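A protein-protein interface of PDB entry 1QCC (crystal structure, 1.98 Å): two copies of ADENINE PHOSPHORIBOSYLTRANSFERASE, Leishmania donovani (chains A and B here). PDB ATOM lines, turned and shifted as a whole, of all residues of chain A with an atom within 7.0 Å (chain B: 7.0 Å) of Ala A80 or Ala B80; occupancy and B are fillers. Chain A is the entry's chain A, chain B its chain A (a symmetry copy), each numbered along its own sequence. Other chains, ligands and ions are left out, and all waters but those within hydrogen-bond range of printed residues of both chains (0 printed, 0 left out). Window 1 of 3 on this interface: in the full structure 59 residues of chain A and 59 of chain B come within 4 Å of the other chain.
Asp A79 touches Ala B80, and with the chains exchanged Ala A80 touches Asp B79. Ala B80 touches its own counterpart, Ala A80. Phe B83 touches its own counterpart, Phe A83. Phe A83 touches Leu B84, and with the chains exchanged Leu A84 touches Phe B83. Positions printed for both chains: 77, 78, 79, 80, 81, 82, 83, 84, 85, 100, 101, 128, 145 and 146. Of the 12 pairs that touch across the chains among the printed residues, 12 have their exchanged pair printed and touching as well.
Of chain B, only Asp B79 (3.6 Å), Ala B80 (3.6 Å), Phe B83 (3.6 Å) and Arg B101 (3.7 Å) come within 4 Å of Ala A80. Ala B80 touches just these residues of chain A: Asp A79 (3.6 Å), Ala A80 (3.6 Å), Phe A83 (3.6 Å) and Arg A101 (3.7 Å). Of the printed residues of chain B, Arg A101 touches Ala B80 (3.7 Å) and Arg B81 (3.7 Å). Printed residues of chain A within 4 Å of Phe B83: Ala A80 (3.6 Å), Phe A83 (3.1 Å) and Leu A84 (3.5 Å). Printed residues of chain B within 4 Å of Arg A81: Arg B101 (3.7 Å). Of the printed residues of chain A, Asp B79 touches Ala A80. Of the printed residues of chain A, Arg B81 touches Arg A101 (3.7 Å). Gly B82 touches none of the printed residues of chain A. The nearest residue of chain B that does not touch Ala A80 is Leu B84 (6.5 Å). The nearest printed residue of chain A that does not touch Leu B84 is Leu A84 (5.6 Å).
O of Phe B83 lies close to O of Phe A83, at 3.1 Å.
Hydrophobic or aromatic side chains of chain A within 4 Å of the printed part of chain B: Ala A80, Phe A83 and Leu A84. Of the 14 printed residues of chain B, 6 touch a printed residue of chain A. Hydrophobic or aromatic side chains of chain B within 4 Å of the printed part of chain A: Ala B80, Phe B83 and Leu B84. Among the printed residues, no Asp or Glu carboxylate lies within 4 Å of a Lys or Arg side-chain nitrogen of the other chain.
O of Met A100 sits at hydrogen-bond distance from N of Asp A79. OD2 of Asp A79 is in salt-bridge range of NE of Arg A101 (2.7 Å). OD1 of Asp A146 lies within salt-bridge range of NE of Arg A81 (2.9 Å). The backbone NH of Asp B79 lies within hydrogen-bond range of the backbone carbonyl oxygen of Met B100. NE of Arg B101 is in salt-bridge range of OD2 of Asp B79 (2.7 Å). OD1 of Asp B146 lies within salt-bridge range of NE of Arg B81.
Among the printed residues, merely in contact across the chains: Phe A83 with Leu B84 (3.5 Å), Leu A84 with Phe B83 (3.5 Å), Ala A80 with Asp B79 (3.6 Å), Asp A79 with Ala B80 (3.6 Å), Ala A80 with Ala B80 (3.6 Å), Phe A83 with Ala B80 (3.6 Å), Ala A80 with Phe B83 (3.6 Å), Ala A80 with Arg B101 (3.7 Å), Arg A101 with Ala B80 (3.7 Å), Arg A101 with Arg B81 (3.7 Å) and Arg A81 with Arg B101 (3.7 Å).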
ATOM      1  N   GLY A  77       0.775  18.561  22.558  1.00  0.00           N
ATOM      2  CA  GLY A  77       1.032  18.497  21.127  1.00  0.00           C
ATOM      3  C   GLY A  77       0.341  19.602  20.355  1.00  0.00           C
ATOM      4  O   GLY A  77      -0.773  20.007  20.703  1.00  0.00           O
ATOM      5  N   PHE A  78       0.995  20.065  19.290  1.00  0.00           N
ATOM      6  CA  PHE A  78       0.479  21.145  18.450  1.00  0.00           C
ATOM      7  C   PHE A  78      -0.437  20.628  17.331  1.00  0.00           C
ATOM      8  O   PHE A  78      -0.144  19.616  16.698  1.00  0.00           O
ATOM      9  CB  PHE A  78       1.643  21.940  17.830  1.00  0.00           C
ATOM     10  CG  PHE A  78       2.597  22.555  18.838  1.00  0.00           C
ATOM     11  CD1 PHE A  78       2.394  22.410  20.211  1.00  0.00           C
ATOM     12  CD2 PHE A  78       3.711  23.268  18.402  1.00  0.00           C
ATOM     13  CE1 PHE A  78       3.290  22.965  21.135  1.00  0.00           C
ATOM     14  CE2 PHE A  78       4.611  23.825  19.310  1.00  0.00           C
ATOM     15  CZ  PHE A  78       4.400  23.672  20.681  1.00  0.00           C
ATOM     16  N   ASP A  79      -1.529  21.346  17.083  1.00  0.00           N
ATOM     17  CA  ASP A  79      -2.507  21.002  16.047  1.00  0.00           C
ATOM     18  C   ASP A  79      -1.893  21.304  14.670  1.00  0.00           C
ATOM     19  O   ASP A  79      -1.536  22.451  14.392  1.00  0.00           O
ATOM     20  CB  ASP A  79      -3.757  21.863  16.282  1.00  0.00           C
ATOM     21  CG  ASP A  79      -4.951  21.479  15.405  1.00  0.00           C
ATOM     22  OD1 ASP A  79      -4.855  20.617  14.509  1.00  0.00           O
ATOM     23  OD2 ASP A  79      -6.024  22.071  15.630  1.00  0.00           O
ATOM     24  N   ALA A  80      -1.708  20.292  13.821  1.00  0.00           N
ATOM     25  CA  ALA A  80      -2.297  18.963  13.952  1.00  0.00           C
ATOM     26  C   ALA A  80      -1.209  17.893  13.906  1.00  0.00           C
ATOM     27  O   ALA A  80      -1.416  16.755  14.332  1.00  0.00           O
ATOM     28  CB  ALA A  80      -3.288  18.720  12.799  1.00  0.00           C
ATOM     29  N   ARG A  81      -0.048  18.263  13.382  1.00  0.00           N
ATOM     30  CA  ARG A  81       1.043  17.319  13.231  1.00  0.00           C
ATOM     31  C   ARG A  81       1.660  16.837  14.540  1.00  0.00           C
ATOM     32  O   ARG A  81       2.239  15.752  14.594  1.00  0.00           O
ATOM     33  CB  ARG A  81       2.059  17.859  12.216  1.00  0.00           C
ATOM     34  CG  ARG A  81       1.344  18.279  10.909  1.00  0.00           C
ATOM     35  CD  ARG A  81       2.255  18.631   9.743  1.00  0.00           C
ATOM     36  NE  ARG A  81       3.199  19.693  10.062  1.00  0.00           N
ATOM     37  CZ  ARG A  81       3.495  20.715   9.263  1.00  0.00           C
ATOM     38  NH1 ARG A  81       4.383  21.614   9.659  1.00  0.00           N
ATOM     39  NH2 ARG A  81       2.877  20.871   8.102  1.00  0.00           N
ATOM     40  N   GLY A  82       1.465  17.603  15.608  1.00  0.00           N
ATOM     41  CA  GLY A  82       1.969  17.195  16.906  1.00  0.00           C
ATOM     42  C   GLY A  82       1.076  16.091  17.462  1.00  0.00           C
ATOM     43  O   GLY A  82       1.491  15.310  18.321  1.00  0.00           O
ATOM     44  N   PHE A  83      -0.162  16.041  16.973  1.00  0.00           N
ATOM     45  CA  PHE A  83      -1.149  15.032  17.381  1.00  0.00           C
ATOM     46  C   PHE A  83      -0.718  13.648  16.892  1.00  0.00           C
ATOM     47  O   PHE A  83      -1.130  12.625  17.432  1.00  0.00           O
ATOM     48  CB  PHE A  83      -2.525  15.337  16.762  1.00  0.00           C
ATOM     49  CG  PHE A  83      -3.214  16.558  17.322  1.00  0.00           C
ATOM     50  CD1 PHE A  83      -2.601  17.369  18.274  1.00  0.00           C
ATOM     51  CD2 PHE A  83      -4.498  16.891  16.887  1.00  0.00           C
ATOM     52  CE1 PHE A  83      -3.255  18.496  18.788  1.00  0.00           C
ATOM     53  CE2 PHE A  83      -5.158  18.013  17.394  1.00  0.00           C
ATOM     54  CZ  PHE A  83      -4.530  18.818  18.349  1.00  0.00           C
ATOM     55  N   LEU A  84       0.106  13.629  15.852  1.00  0.00           N
ATOM     56  CA  LEU A  84       0.586  12.391  15.255  1.00  0.00           C
ATOM     57  C   LEU A  84       1.611  11.632  16.086  1.00  0.00           C
ATOM     58  O   LEU A  84       1.703  10.412  15.979  1.00  0.00           O
ATOM     59  CB  LEU A  84       1.192  12.690  13.876  1.00  0.00           C
ATOM     60  CG  LEU A  84       0.274  13.351  12.845  1.00  0.00           C
ATOM     61  CD1 LEU A  84       1.085  13.960  11.714  1.00  0.00           C
ATOM     62  CD2 LEU A  84      -0.712  12.335  12.327  1.00  0.00           C
ATOM     63  N   PHE A  85       2.364  12.348  16.918  1.00  0.00           N
ATOM     64  CA  PHE A  85       3.424  11.730  17.710  1.00  0.00           C
ATOM     65  C   PHE A  85       3.207  11.697  19.223  1.00  0.00           C
ATOM     66  O   PHE A  85       3.658  10.769  19.906  1.00  0.00           O
ATOM     67  CB  PHE A  85       4.757  12.422  17.392  1.00  0.00           C
ATOM     68  CG  PHE A  85       5.095  12.435  15.925  1.00  0.00           C
ATOM     69  CD1 PHE A  85       5.577  11.289  15.295  1.00  0.00           C
ATOM     70  CD2 PHE A  85       4.875  13.577  15.157  1.00  0.00           C
ATOM     71  CE1 PHE A  85       5.826  11.274  13.924  1.00  0.00           C
ATOM     72  CE2 PHE A  85       5.123  13.573  13.787  1.00  0.00           C
ATOM     73  CZ  PHE A  85       5.598  12.418  13.169  1.00  0.00           C
ATOM     74  N   MET A 100      -3.046  21.628  21.863  1.00  0.00           N
ATOM     75  CA  MET A 100      -2.929  23.067  21.657  1.00  0.00           C
ATOM     76  C   MET A 100      -3.563  23.325  20.287  1.00  0.00           C
ATOM     77  O   MET A 100      -3.081  22.840  19.255  1.00  0.00           O
ATOM     78  CB  MET A 100      -1.476  23.557  21.696  1.00  0.00           C
ATOM     79  CG  MET A 100      -1.383  25.091  21.621  1.00  0.00           C
ATOM     80  SD  MET A 100       0.262  25.838  21.742  1.00  0.00           S
ATOM     81  CE  MET A 100       0.891  25.564  20.106  1.00  0.00           C
ATOM     82  N   ARG A 101      -4.686  24.037  20.293  1.00  0.00           N
ATOM     83  CA  ARG A 101      -5.415  24.332  19.064  1.00  0.00           C
ATOM     84  C   ARG A 101      -5.920  25.772  19.029  1.00  0.00           C
ATOM     85  O   ARG A 101      -5.876  26.476  20.036  1.00  0.00           O
ATOM     86  CB  ARG A 101      -6.638  23.416  18.955  1.00  0.00           C
ATOM     87  CG  ARG A 101      -6.443  21.982  19.420  1.00  0.00           C
ATOM     88  CD  ARG A 101      -7.593  21.100  18.942  1.00  0.00           C
ATOM     89  NE  ARG A 101      -7.616  21.012  17.485  1.00  0.00           N
ATOM     90  CZ  ARG A 101      -8.478  20.285  16.781  1.00  0.00           C
ATOM     91  NH1 ARG A 101      -8.403  20.273  15.455  1.00  0.00           N
ATOM     92  NH2 ARG A 101      -9.418  19.579  17.394  1.00  0.00           N
ATOM     93  N   MET A 128      -2.986  30.613  19.693  1.00  0.00           N
ATOM     94  CA  MET A 128      -3.290  29.233  20.066  1.00  0.00           C
ATOM     95  C   MET A 128      -3.819  29.121  21.501  1.00  0.00           C
ATOM     96  O   MET A 128      -3.576  29.996  22.337  1.00  0.00           O
ATOM     97  CB  MET A 128      -2.052  28.353  19.873  1.00  0.00           C
ATOM     98  CG  MET A 128      -1.540  28.296  18.434  1.00  0.00           C
ATOM     99  SD  MET A 128      -2.649  27.427  17.321  1.00  0.00           S
ATOM    100  CE  MET A 128      -2.255  25.758  17.740  1.00  0.00           C
ATOM    101  N   ASP A 145       5.888  18.640  18.350  1.00  0.00           N
ATOM    102  CA  ASP A 145       5.405  19.006  17.021  1.00  0.00           C
ATOM    103  C   ASP A 145       6.376  18.338  16.045  1.00  0.00           C
ATOM    104  O   ASP A 145       7.453  17.884  16.448  1.00  0.00           O
ATOM    105  CB  ASP A 145       5.434  20.535  16.854  1.00  0.00           C
ATOM    106  CG  ASP A 145       4.630  21.026  15.652  1.00  0.00           C
ATOM    107  OD1 ASP A 145       4.612  22.252  15.419  1.00  0.00           O
ATOM    108  OD2 ASP A 145       4.015  20.209  14.938  1.00  0.00           O
ATOM    109  N   ASP A 146       6.011  18.258  14.772  1.00  0.00           N
ATOM    110  CA  ASP A 146       6.899  17.620  13.811  1.00  0.00           C
ATOM    111  C   ASP A 146       8.123  18.446  13.399  1.00  0.00           C
ATOM    112  O   ASP A 146       9.247  17.946  13.422  1.00  0.00           O
ATOM    113  CB  ASP A 146       6.120  17.131  12.581  1.00  0.00           C
ATOM    114  CG  ASP A 146       5.633  18.262  11.685  1.00  0.00           C
ATOM    115  OD1 ASP A 146       5.559  18.028  10.459  1.00  0.00           O
ATOM    116  OD2 ASP A 146       5.315  19.366  12.188  1.00  0.00           O
ATOM    117  N   GLY B  77      -6.434   8.189   8.897  1.00  0.00           N
ATOM    118  CA  GLY B  77      -7.037   9.035   9.917  1.00  0.00           C
ATOM    119  C   GLY B  77      -7.438  10.397   9.392  1.00  0.00           C
ATOM    120  O   GLY B  77      -6.753  10.964   8.532  1.00  0.00           O
ATOM    121  N   PHE B  78      -8.532  10.931   9.933  1.00  0.00           N
ATOM    122  CA  PHE B  78      -9.068  12.229   9.522  1.00  0.00           C
ATOM    123  C   PHE B  78      -8.439  13.393  10.301  1.00  0.00           C
ATOM    124  O   PHE B  78      -8.245  13.306  11.512  1.00  0.00           O
ATOM    125  CB  PHE B  78     -10.597  12.258   9.709  1.00  0.00           C
ATOM    126  CG  PHE B  78     -11.347  11.185   8.941  1.00  0.00           C
ATOM    127  CD1 PHE B  78     -10.678  10.274   8.124  1.00  0.00           C
ATOM    128  CD2 PHE B  78     -12.732  11.082   9.056  1.00  0.00           C
ATOM    129  CE1 PHE B  78     -11.377   9.275   7.433  1.00  0.00           C
ATOM    130  CE2 PHE B  78     -13.440  10.093   8.376  1.00  0.00           C
ATOM    131  CZ  PHE B  78     -12.761   9.186   7.562  1.00  0.00           C
ATOM    132  N   ASP B  79      -8.146  14.484   9.597  1.00  0.00           N
ATOM    133  CA  ASP B  79      -7.549  15.688  10.181  1.00  0.00           C
ATOM    134  C   ASP B  79      -8.615  16.412  11.019  1.00  0.00           C
ATOM    135  O   ASP B  79      -9.656  16.807  10.486  1.00  0.00           O
ATOM    136  CB  ASP B  79      -7.073  16.580   9.024  1.00  0.00           C
ATOM    137  CG  ASP B  79      -6.243  17.786   9.469  1.00  0.00           C
ATOM    138  OD1 ASP B  79      -6.078  18.060  10.674  1.00  0.00           O
ATOM    139  OD2 ASP B  79      -5.740  18.482   8.567  1.00  0.00           O
ATOM    140  N   ALA B  80      -8.411  16.544  12.331  1.00  0.00           N
ATOM    141  CA  ALA B  80      -7.139  16.328  13.012  1.00  0.00           C
ATOM    142  C   ALA B  80      -7.310  15.323  14.149  1.00  0.00           C
ATOM    143  O   ALA B  80      -6.339  14.735  14.631  1.00  0.00           O
ATOM    144  CB  ALA B  80      -6.629  17.659  13.592  1.00  0.00           C
ATOM    145  N   ARG B  81      -8.550  15.132  14.578  1.00  0.00           N
ATOM    146  CA  ARG B  81      -8.832  14.246  15.692  1.00  0.00           C
ATOM    147  C   ARG B  81      -8.581  12.767  15.414  1.00  0.00           C
ATOM    148  O   ARG B  81      -8.338  11.992  16.338  1.00  0.00           O
ATOM    149  CB  ARG B  81     -10.224  14.555  16.261  1.00  0.00           C
ATOM    150  CG  ARG B  81     -10.364  16.069  16.551  1.00  0.00           C
ATOM    151  CD  ARG B  81     -11.612  16.481  17.315  1.00  0.00           C
ATOM    152  NE  ARG B  81     -12.844  16.066  16.656  1.00  0.00           N
ATOM    153  CZ  ARG B  81     -13.927  16.826  16.519  1.00  0.00           C
ATOM    154  NH1 ARG B  81     -14.993  16.332  15.908  1.00  0.00           N
ATOM    155  NH2 ARG B  81     -13.934  18.083  16.935  1.00  0.00           N
ATOM    156  N   GLY B  82      -8.562  12.397  14.138  1.00  0.00           N
ATOM    157  CA  GLY B  82      -8.277  11.020  13.778  1.00  0.00           C
ATOM    158  C   GLY B  82      -6.782  10.763  13.939  1.00  0.00           C
ATOM    159  O   GLY B  82      -6.346   9.620  14.090  1.00  0.00           O
ATOM    160  N   PHE B  83      -5.998  11.839  13.888  1.00  0.00           N
ATOM    161  CA  PHE B  83      -4.537  11.778  14.043  1.00  0.00           C
ATOM    162  C   PHE B  83      -4.176  11.371  15.472  1.00  0.00           C
ATOM    163  O   PHE B  83      -3.089  10.868  15.735  1.00  0.00           O
ATOM    164  CB  PHE B  83      -3.906  13.157  13.777  1.00  0.00           C
ATOM    165  CG  PHE B  83      -3.957  13.609  12.337  1.00  0.00           C
ATOM    166  CD1 PHE B  83      -4.592  12.850  11.357  1.00  0.00           C
ATOM    167  CD2 PHE B  83      -3.351  14.809  11.965  1.00  0.00           C
ATOM    168  CE1 PHE B  83      -4.627  13.281  10.024  1.00  0.00           C
ATOM    169  CE2 PHE B  83      -3.381  15.247  10.638  1.00  0.00           C
ATOM    170  CZ  PHE B  83      -4.024  14.476   9.665  1.00  0.00           C
ATOM    171  N   LEU B  84      -5.099  11.614  16.396  1.00  0.00           N
ATOM    172  CA  LEU B  84      -4.897  11.308  17.805  1.00  0.00           C
ATOM    173  C   LEU B  84      -4.931   9.826  18.152  1.00  0.00           C
ATOM    174  O   LEU B  84      -4.299   9.409  19.120  1.00  0.00           O
ATOM    175  CB  LEU B  84      -5.956  12.036  18.643  1.00  0.00           C
ATOM    176  CG  LEU B  84      -6.005  13.561  18.524  1.00  0.00           C
ATOM    177  CD1 LEU B  84      -7.324  14.100  19.052  1.00  0.00           C
ATOM    178  CD2 LEU B  84      -4.835  14.159  19.262  1.00  0.00           C
ATOM    179  N   PHE B  85      -5.651   9.035  17.359  1.00  0.00           N
ATOM    180  CA  PHE B  85      -5.808   7.611  17.640  1.00  0.00           C
ATOM    181  C   PHE B  85      -5.150   6.649  16.651  1.00  0.00           C
ATOM    182  O   PHE B  85      -4.708   5.557  17.030  1.00  0.00           O
ATOM    183  CB  PHE B  85      -7.303   7.286  17.766  1.00  0.00           C
ATOM    184  CG  PHE B  85      -8.023   8.135  18.780  1.00  0.00           C
ATOM    185  CD1 PHE B  85      -7.887   7.884  20.144  1.00  0.00           C
ATOM    186  CD2 PHE B  85      -8.789   9.226  18.373  1.00  0.00           C
ATOM    187  CE1 PHE B  85      -8.494   8.710  21.089  1.00  0.00           C
ATOM    188  CE2 PHE B  85      -9.402  10.054  19.310  1.00  0.00           C
ATOM    189  CZ  PHE B  85      -9.252   9.796  20.671  1.00  0.00           C
ATOM    190  N   MET B 100      -5.691  12.081   5.932  1.00  0.00           N
ATOM    191  CA  MET B 100      -6.707  12.675   5.070  1.00  0.00           C
ATOM    192  C   MET B 100      -6.829  14.128   5.541  1.00  0.00           C
ATOM    193  O   MET B 100      -7.217  14.401   6.684  1.00  0.00           O
ATOM    194  CB  MET B 100      -8.056  11.949   5.154  1.00  0.00           C
ATOM    195  CG  MET B 100      -9.069  12.498   4.135  1.00  0.00           C
ATOM    196  SD  MET B 100     -10.689  11.692   4.045  1.00  0.00           S
ATOM    197  CE  MET B 100     -11.502  12.383   5.461  1.00  0.00           C
ATOM    198  N   ARG B 101      -6.430  15.053   4.674  1.00  0.00           N
ATOM    199  CA  ARG B 101      -6.460  16.475   5.000  1.00  0.00           C
ATOM    200  C   ARG B 101      -6.966  17.319   3.833  1.00  0.00           C
ATOM    201  O   ARG B 101      -7.103  16.826   2.715  1.00  0.00           O
ATOM    202  CB  ARG B 101      -5.047  16.959   5.336  1.00  0.00           C
ATOM    203  CG  ARG B 101      -4.182  15.994   6.132  1.00  0.00           C
ATOM    204  CD  ARG B 101      -2.959  16.711   6.697  1.00  0.00           C
ATOM    205  NE  ARG B 101      -3.348  17.734   7.662  1.00  0.00           N
ATOM    206  CZ  ARG B 101      -2.501  18.495   8.349  1.00  0.00           C
ATOM    207  NH1 ARG B 101      -2.968  19.393   9.208  1.00  0.00           N
ATOM    208  NH2 ARG B 101      -1.193  18.368   8.173  1.00  0.00           N
ATOM    209  N   MET B 128     -11.819  16.818   0.887  1.00  0.00           N
ATOM    210  CA  MET B 128     -10.648  16.240   1.544  1.00  0.00           C
ATOM    211  C   MET B 128      -9.740  15.493   0.561  1.00  0.00           C
ATOM    212  O   MET B 128     -10.181  15.063  -0.509  1.00  0.00           O
ATOM    213  CB  MET B 128     -11.090  15.318   2.684  1.00  0.00           C
ATOM    214  CG  MET B 128     -11.887  16.017   3.786  1.00  0.00           C
ATOM    215  SD  MET B 128     -10.902  17.168   4.751  1.00  0.00           S
ATOM    216  CE  MET B 128     -10.057  16.033   5.806  1.00  0.00           C
ATOM    217  N   ASP B 145     -11.567   8.152  13.082  1.00  0.00           N
ATOM    218  CA  ASP B 145     -11.852   9.523  13.499  1.00  0.00           C
ATOM    219  C   ASP B 145     -12.472   9.398  14.892  1.00  0.00           C
ATOM    220  O   ASP B 145     -12.862   8.300  15.305  1.00  0.00           O
ATOM    221  CB  ASP B 145     -12.845  10.174  12.519  1.00  0.00           C
ATOM    222  CG  ASP B 145     -12.928  11.692  12.665  1.00  0.00           C
ATOM    223  OD1 ASP B 145     -13.726  12.308  11.929  1.00  0.00           O
ATOM    224  OD2 ASP B 145     -12.211  12.278  13.500  1.00  0.00           O
ATOM    225  N   ASP B 146     -12.558  10.497  15.629  1.00  0.00           N
ATOM    226  CA  ASP B 146     -13.130  10.422  16.965  1.00  0.00           C
ATOM    227  C   ASP B 146     -14.656  10.277  17.019  1.00  0.00           C
ATOM    228  O   ASP B 146     -15.172   9.406  17.716  1.00  0.00           O
ATOM    229  CB  ASP B 146     -12.653  11.593  17.836  1.00  0.00           C
ATOM    230  CG  ASP B 146     -13.258  12.931  17.434  1.00  0.00           C
ATOM    231  OD1 ASP B 146     -13.450  13.768  18.342  1.00  0.00           O
ATOM    232  OD2 ASP B 146     -13.530  13.159  16.230  1.00  0.00           O
